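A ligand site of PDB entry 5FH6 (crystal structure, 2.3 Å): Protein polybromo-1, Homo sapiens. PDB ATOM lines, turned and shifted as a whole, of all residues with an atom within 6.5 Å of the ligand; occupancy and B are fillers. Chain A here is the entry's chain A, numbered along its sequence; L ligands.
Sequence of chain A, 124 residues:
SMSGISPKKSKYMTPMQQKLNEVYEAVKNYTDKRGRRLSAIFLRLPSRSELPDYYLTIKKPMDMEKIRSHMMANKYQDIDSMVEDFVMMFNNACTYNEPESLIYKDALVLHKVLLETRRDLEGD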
ATOM      1  N   ILE A  41      26.477 -31.657 -27.738  1.00  0.00           N
ATOM      2  CA  ILE A  41      25.132 -32.108 -27.408  1.00  0.00           C
ATOM      3  C   ILE A  41      24.076 -31.242 -28.101  1.00  0.00           C
ATOM      4  O   ILE A  41      22.959 -31.675 -28.343  1.00  0.00           O
ATOM      5  CB  ILE A  41      24.892 -32.106 -25.874  1.00  0.00           C
ATOM      6  CG1 ILE A  41      23.648 -32.923 -25.508  1.00  0.00           C
ATOM      7  CG2 ILE A  41      24.785 -30.685 -25.340  1.00  0.00           C
ATOM      8  CD1 ILE A  41      23.745 -34.393 -25.861  1.00  0.00           C
ATOM      9  N   PHE A  42      24.457 -30.010 -28.448  1.00  0.00           N
ATOM     10  CA  PHE A  42      23.529 -29.049 -29.029  1.00  0.00           C
ATOM     11  C   PHE A  42      23.462 -29.061 -30.544  1.00  0.00           C
ATOM     12  O   PHE A  42      22.662 -28.330 -31.125  1.00  0.00           O
ATOM     13  CB  PHE A  42      23.894 -27.632 -28.590  1.00  0.00           C
ATOM     14  CG  PHE A  42      23.800 -27.406 -27.116  1.00  0.00           C
ATOM     15  CD1 PHE A  42      22.573 -27.434 -26.475  1.00  0.00           C
ATOM     16  CD2 PHE A  42      24.932 -27.137 -26.369  1.00  0.00           C
ATOM     17  CE1 PHE A  42      22.470 -27.223 -25.115  1.00  0.00           C
ATOM     18  CE2 PHE A  42      24.847 -26.924 -25.009  1.00  0.00           C
ATOM     19  CZ  PHE A  42      23.610 -26.964 -24.379  1.00  0.00           C
ATOM     20  N   LEU A  43      24.279 -29.887 -31.190  1.00  0.00           N
ATOM     21  CA  LEU A  43      24.380 -29.795 -32.637  1.00  0.00           C
ATOM     22  C   LEU A  43      23.051 -30.139 -33.271  1.00  0.00           C
ATOM     23  O   LEU A  43      22.519 -29.375 -34.083  1.00  0.00           O
ATOM     24  CB  LEU A  43      25.454 -30.746 -33.180  1.00  0.00           C
ATOM     25  CG  LEU A  43      26.877 -30.240 -32.972  1.00  0.00           C
ATOM     26  CD1 LEU A  43      27.926 -31.248 -33.450  1.00  0.00           C
ATOM     27  CD2 LEU A  43      27.070 -28.886 -33.630  1.00  0.00           C
ATOM     28  N   ARG A  44      22.529 -31.298 -32.899  1.00  0.00           N
ATOM     29  CA  ARG A  44      21.227 -31.694 -33.467  1.00  0.00           C
ATOM     30  C   ARG A  44      20.376 -32.517 -32.562  1.00  0.00           C
ATOM     31  O   ARG A  44      20.841 -33.490 -32.013  1.00  0.00           O
ATOM     32  CB  ARG A  44      21.434 -32.456 -34.816  1.00  0.00           C
ATOM     33  CG  ARG A  44      20.079 -32.849 -35.716  1.00  0.00           C
ATOM     34  CD  ARG A  44      20.323 -33.519 -37.095  1.00  0.00           C
ATOM     35  NE  ARG A  44      19.271 -33.092 -38.016  1.00  0.00           N
ATOM     36  CZ  ARG A  44      19.147 -33.426 -39.288  1.00  0.00           C
ATOM     37  NH1 ARG A  44      19.917 -34.254 -40.161  1.00  0.00           N
ATOM     38  NH2 ARG A  44      18.111 -32.876 -39.808  1.00  0.00           N
ATOM     39  N   LEU A  45      19.088 -32.211 -32.503  1.00  0.00           N
ATOM     40  CA  LEU A  45      18.166 -33.006 -31.703  1.00  0.00           C
ATOM     41  C   LEU A  45      17.765 -34.326 -32.352  1.00  0.00           C
ATOM     42  O   LEU A  45      17.597 -34.421 -33.572  1.00  0.00           O
ATOM     43  CB  LEU A  45      16.882 -32.221 -31.397  1.00  0.00           C
ATOM     44  CG  LEU A  45      16.811 -31.295 -30.188  1.00  0.00           C
ATOM     45  CD1 LEU A  45      15.609 -30.391 -30.320  1.00  0.00           C
ATOM     46  CD2 LEU A  45      16.709 -32.116 -28.906  1.00  0.00           C
ATOM     47  N   PRO A  46      17.607 -35.377 -31.524  1.00  0.00           N
ATOM     48  CA  PRO A  46      17.034 -36.655 -31.936  1.00  0.00           C
ATOM     49  C   PRO A  46      15.618 -36.416 -32.443  1.00  0.00           C
ATOM     50  O   PRO A  46      14.996 -35.424 -32.059  1.00  0.00           O
ATOM     51  CB  PRO A  46      17.044 -37.495 -30.644  1.00  0.00           C
ATOM     52  CG  PRO A  46      17.152 -36.493 -29.535  1.00  0.00           C
ATOM     53  CD  PRO A  46      17.998 -35.392 -30.104  1.00  0.00           C
ATOM     54  N   LEU A  51      12.439 -38.998 -29.051  1.00  0.00           N
ATOM     55  CA  LEU A  51      12.350 -38.234 -27.823  1.00  0.00           C
ATOM     56  C   LEU A  51      11.101 -37.353 -27.804  1.00  0.00           C
ATOM     57  O   LEU A  51      11.203 -36.120 -27.826  1.00  0.00           O
ATOM     58  CB  LEU A  51      13.603 -37.379 -27.642  1.00  0.00           C
ATOM     59  CG  LEU A  51      14.051 -37.051 -26.216  1.00  0.00           C
ATOM     60  CD1 LEU A  51      14.504 -38.318 -25.508  1.00  0.00           C
ATOM     61  CD2 LEU A  51      15.180 -36.027 -26.246  1.00  0.00           C
ATOM     62  N   TYR A  54      10.552 -34.431 -25.205  1.00  0.00           N
ATOM     63  CA  TYR A  54      11.185 -33.135 -25.410  1.00  0.00           C
ATOM     64  C   TYR A  54      10.253 -32.215 -26.201  1.00  0.00           C
ATOM     65  O   TYR A  54      10.140 -31.031 -25.882  1.00  0.00           O
ATOM     66  CB  TYR A  54      12.530 -33.276 -26.141  1.00  0.00           C
ATOM     67  CG  TYR A  54      13.316 -31.978 -26.157  1.00  0.00           C
ATOM     68  CD1 TYR A  54      14.110 -31.636 -25.078  1.00  0.00           C
ATOM     69  CD2 TYR A  54      13.253 -31.106 -27.233  1.00  0.00           C
ATOM     70  CE1 TYR A  54      14.828 -30.458 -25.058  1.00  0.00           C
ATOM     71  CE2 TYR A  54      13.965 -29.924 -27.229  1.00  0.00           C
ATOM     72  CZ  TYR A  54      14.761 -29.606 -26.143  1.00  0.00           C
ATOM     73  OH  TYR A  54      15.472 -28.430 -26.116  1.00  0.00           O
ATOM     74  N   ILE A  58       8.674 -28.914 -24.473  1.00  0.00           N
ATOM     75  CA  ILE A  58       9.326 -27.701 -24.963  1.00  0.00           C
ATOM     76  C   ILE A  58       8.545 -27.213 -26.167  1.00  0.00           C
ATOM     77  O   ILE A  58       8.331 -27.949 -27.131  1.00  0.00           O
ATOM     78  CB  ILE A  58      10.806 -27.963 -25.355  1.00  0.00           C
ATOM     79  CG1 ILE A  58      11.631 -28.378 -24.132  1.00  0.00           C
ATOM     80  CG2 ILE A  58      11.412 -26.725 -25.986  1.00  0.00           C
ATOM     81  CD1 ILE A  58      11.774 -27.306 -23.077  1.00  0.00           C
ATOM     82  N   MET A  62      14.715 -26.205 -30.751  1.00  0.00           N
ATOM     83  CA  MET A  62      15.785 -25.606 -31.551  1.00  0.00           C
ATOM     84  C   MET A  62      17.106 -26.364 -31.423  1.00  0.00           C
ATOM     85  O   MET A  62      17.475 -26.788 -30.328  1.00  0.00           O
ATOM     86  CB  MET A  62      15.978 -24.144 -31.131  1.00  0.00           C
ATOM     87  CG  MET A  62      16.833 -23.298 -32.065  1.00  0.00           C
ATOM     88  SD  MET A  62      16.227 -23.294 -33.747  1.00  0.00           S
ATOM     89  CE  MET A  62      14.799 -22.211 -33.621  1.00  0.00           C
ATOM     90  N   ASP A  63      17.827 -26.533 -32.525  1.00  0.00           N
ATOM     91  CA  ASP A  63      19.202 -27.026 -32.458  1.00  0.00           C
ATOM     92  C   ASP A  63      20.101 -26.265 -33.440  1.00  0.00           C
ATOM     93  O   ASP A  63      19.628 -25.411 -34.178  1.00  0.00           O
ATOM     94  CB  ASP A  63      19.239 -28.556 -32.695  1.00  0.00           C
ATOM     95  CG  ASP A  63      18.755 -28.973 -34.078  1.00  0.00           C
ATOM     96  OD1 ASP A  63      18.734 -28.139 -34.996  1.00  0.00           O
ATOM     97  OD2 ASP A  63      18.371 -30.153 -34.229  1.00  0.00           O
ATOM     98  N   MET A  64      21.394 -26.577 -33.446  1.00  0.00           N
ATOM     99  CA  MET A  64      22.350 -25.733 -34.140  1.00  0.00           C
ATOM    100  C   MET A  64      22.360 -25.922 -35.649  1.00  0.00           C
ATOM    101  O   MET A  64      22.561 -24.961 -36.400  1.00  0.00           O
ATOM    102  CB  MET A  64      23.748 -25.972 -33.583  1.00  0.00           C
ATOM    103  CG  MET A  64      24.025 -25.220 -32.298  1.00  0.00           C
ATOM    104  SD  MET A  64      25.655 -25.531 -31.624  1.00  0.00           S
ATOM    105  CE  MET A  64      26.617 -24.326 -32.508  1.00  0.00           C
ATOM    106  N   MET A  89      17.234 -21.624 -27.943  1.00  0.00           N
ATOM    107  CA  MET A  89      17.703 -23.003 -27.828  1.00  0.00           C
ATOM    108  C   MET A  89      18.258 -23.308 -26.442  1.00  0.00           C
ATOM    109  O   MET A  89      17.971 -24.361 -25.875  1.00  0.00           O
ATOM    110  CB  MET A  89      18.762 -23.308 -28.887  1.00  0.00           C
ATOM    111  CG  MET A  89      19.366 -24.699 -28.755  1.00  0.00           C
ATOM    112  SD  MET A  89      20.744 -25.040 -29.878  1.00  0.00           S
ATOM    113  CE  MET A  89      21.959 -23.883 -29.274  1.00  0.00           C
ATOM    114  N   PHE A  90      19.058 -22.393 -25.902  1.00  0.00           N
ATOM    115  CA  PHE A  90      19.642 -22.568 -24.577  1.00  0.00           C
ATOM    116  C   PHE A  90      18.575 -22.647 -23.491  1.00  0.00           C
ATOM    117  O   PHE A  90      18.608 -23.529 -22.633  1.00  0.00           O
ATOM    118  CB  PHE A  90      20.608 -21.434 -24.264  1.00  0.00           C
ATOM    119  CG  PHE A  90      21.783 -21.363 -25.197  1.00  0.00           C
ATOM    120  CD1 PHE A  90      22.344 -22.522 -25.722  1.00  0.00           C
ATOM    121  CD2 PHE A  90      22.333 -20.142 -25.540  1.00  0.00           C
ATOM    122  CE1 PHE A  90      23.425 -22.454 -26.571  1.00  0.00           C
ATOM    123  CE2 PHE A  90      23.420 -20.072 -26.397  1.00  0.00           C
ATOM    124  CZ  PHE A  90      23.963 -21.229 -26.908  1.00  0.00           C
ATOM    125  N   ASN A  92      15.581 -23.544 -23.818  1.00  0.00           N
ATOM    126  CA  ASN A  92      14.936 -24.840 -23.942  1.00  0.00           C
ATOM    127  C   ASN A  92      15.716 -25.908 -23.185  1.00  0.00           C
ATOM    128  O   ASN A  92      15.145 -26.672 -22.415  1.00  0.00           O
ATOM    129  CB  ASN A  92      14.795 -25.263 -25.411  1.00  0.00           C
ATOM    130  CG  ASN A  92      13.985 -24.284 -26.233  1.00  0.00           C
ATOM    131  OD1 ASN A  92      13.277 -23.432 -25.692  1.00  0.00           O
ATOM    132  ND2 ASN A  92      14.036 -24.446 -27.550  1.00  0.00           N
ATOM    133  N   ALA A  93      17.025 -25.948 -23.432  1.00  0.00           N
ATOM    134  CA  ALA A  93      17.900 -26.919 -22.777  1.00  0.00           C
ATOM    135  C   ALA A  93      17.866 -26.769 -21.273  1.00  0.00           C
ATOM    136  O   ALA A  93      17.847 -27.749 -20.539  1.00  0.00           O
ATOM    137  CB  ALA A  93      19.334 -26.777 -23.293  1.00  0.00           C
ATOM    138  N   CYS A  94      17.837 -25.524 -20.821  1.00  0.00           N
ATOM    139  CA  CYS A  94      17.835 -25.230 -19.398  1.00  0.00           C
ATOM    140  C   CYS A  94      16.459 -25.439 -18.774  1.00  0.00           C
ATOM    141  O   CYS A  94      16.310 -25.423 -17.555  1.00  0.00           O
ATOM    142  CB  CYS A  94      18.306 -23.792 -19.158  1.00  0.00           C
ATOM    143  SG  CYS A  94      20.054 -23.524 -19.466  1.00  0.00           S
ATOM    144  N   TYR A  96      14.369 -28.168 -19.996  1.00  0.00           N
ATOM    145  CA  TYR A  96      14.168 -29.604 -20.078  1.00  0.00           C
ATOM    146  C   TYR A  96      15.128 -30.367 -19.175  1.00  0.00           C
ATOM    147  O   TYR A  96      14.834 -31.451 -18.688  1.00  0.00           O
ATOM    148  CB  TYR A  96      14.334 -30.073 -21.521  1.00  0.00           C
ATOM    149  CG  TYR A  96      14.027 -31.532 -21.726  1.00  0.00           C
ATOM    150  CD1 TYR A  96      12.723 -31.958 -21.935  1.00  0.00           C
ATOM    151  CD2 TYR A  96      15.040 -32.492 -21.713  1.00  0.00           C
ATOM    152  CE1 TYR A  96      12.431 -33.287 -22.123  1.00  0.00           C
ATOM    153  CE2 TYR A  96      14.755 -33.828 -21.898  1.00  0.00           C
ATOM    154  CZ  TYR A  96      13.447 -34.227 -22.099  1.00  0.00           C
ATOM    155  OH  TYR A  96      13.155 -35.556 -22.287  1.00  0.00           O
ATOM    156  N   ASN A  97      16.305 -29.779 -18.963  1.00  0.00           N
ATOM    157  CA  ASN A  97      17.342 -30.377 -18.151  1.00  0.00           C
ATOM    158  C   ASN A  97      17.363 -29.681 -16.790  1.00  0.00           C
ATOM    159  O   ASN A  97      16.994 -28.509 -16.699  1.00  0.00           O
ATOM    160  CB  ASN A  97      18.697 -30.234 -18.839  1.00  0.00           C
ATOM    161  CG  ASN A  97      18.745 -30.919 -20.186  1.00  0.00           C
ATOM    162  OD1 ASN A  97      19.075 -32.105 -20.296  1.00  0.00           O
ATOM    163  ND2 ASN A  97      18.416 -30.171 -21.241  1.00  0.00           N
ATOM    164  N   ILE A 103      24.302 -30.374 -19.447  1.00  0.00           N
ATOM    165  CA  ILE A 103      23.750 -29.694 -20.611  1.00  0.00           C
ATOM    166  C   ILE A 103      23.356 -28.281 -20.198  1.00  0.00           C
ATOM    167  O   ILE A 103      23.648 -27.317 -20.894  1.00  0.00           O
ATOM    168  CB  ILE A 103      22.550 -30.450 -21.167  1.00  0.00           C
ATOM    169  CG1 ILE A 103      22.977 -31.844 -21.613  1.00  0.00           C
ATOM    170  CG2 ILE A 103      21.900 -29.674 -22.316  1.00  0.00           C
ATOM    171  CD1 ILE A 103      21.848 -32.747 -22.002  1.00  0.00           C
HETATM  172  C1  LIG L   1      18.398 -36.120 -23.575  1.00  0.00           C
HETATM  173  C2  LIG L   1      18.707 -37.491 -23.008  1.00  0.00           C
HETATM  174  C3  LIG L   1      18.490 -37.478 -21.505  1.00  0.00           C
HETATM  175  C4  LIG L   1      19.416 -36.440 -20.934  1.00  0.00           C
HETATM  176  C5  LIG L   1      19.094 -35.062 -21.533  1.00  0.00           C
HETATM  177  N1  LIG L   1      19.251 -35.052 -23.008  1.00  0.00           N
HETATM  178  C6  LIG L   1      18.974 -33.838 -23.503  1.00  0.00           C
HETATM  179  C7  LIG L   1      19.254 -33.441 -24.752  1.00  0.00           C
HETATM  180  C8  LIG L   1      19.174 -34.089 -25.961  1.00  0.00           C
HETATM  181  C9  LIG L   1      20.240 -33.300 -26.620  1.00  0.00           C
HETATM  182  N2  LIG L   1      19.516 -32.038 -26.408  1.00  0.00           N
HETATM  183  C10 LIG L   1      18.940 -32.215 -25.194  1.00  0.00           C
HETATM  184  N3  LIG L   1      18.282 -31.130 -24.624  1.00  0.00           N
HETATM  185  C11 LIG L   1      18.140 -29.947 -25.354  1.00  0.00           C
HETATM  186  O1  LIG L   1      17.506 -29.020 -24.874  1.00  0.00           O
HETATM  187  C12 LIG L   1      18.747 -29.834 -26.595  1.00  0.00           C
HETATM  188  C13 LIG L   1      19.466 -30.903 -27.114  1.00  0.00           C
HETATM  189  C14 LIG L   1      20.073 -30.793 -28.368  1.00  0.00           C
HETATM  190  C15 LIG L   1      19.970 -29.601 -29.091  1.00  0.00           C
HETATM  191  C16 LIG L   1      19.252 -28.541 -28.562  1.00  0.00           C
HETATM  192  C17 LIG L   1      18.633 -28.650 -27.316  1.00  0.00           C
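The side-chain hydroxyl (OH) of Tyr 54 sits at hydrogen-bond distance from an oxygen (O1) of the ligand (2.5 Å).
O1 of the ligand lies close to N of Ala 93.
O of Phe 42 lies within hydrogen-bond range of N of Met 64, at 3.2 Å.
The side-chain amide nitrogen (ND2) of Asn 97 lies within hydrogen-bond range of the backbone carbonyl oxygen (O) of Ala 93 (2.6 Å).
The backbone NH of Leu 45 is in hydrogen-bond range of the side-chain carboxylate of Asp 63, 2.8 Å away.
Residues that only touch the ligand: Ile 41, Phe 42, Leu 45, Met 62, Asp 63, Met 89, Asn 92, Asn 97 and Ile 103.
The nearest printed residue that does not touch the ligand is Leu 51 (4.2 Å).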
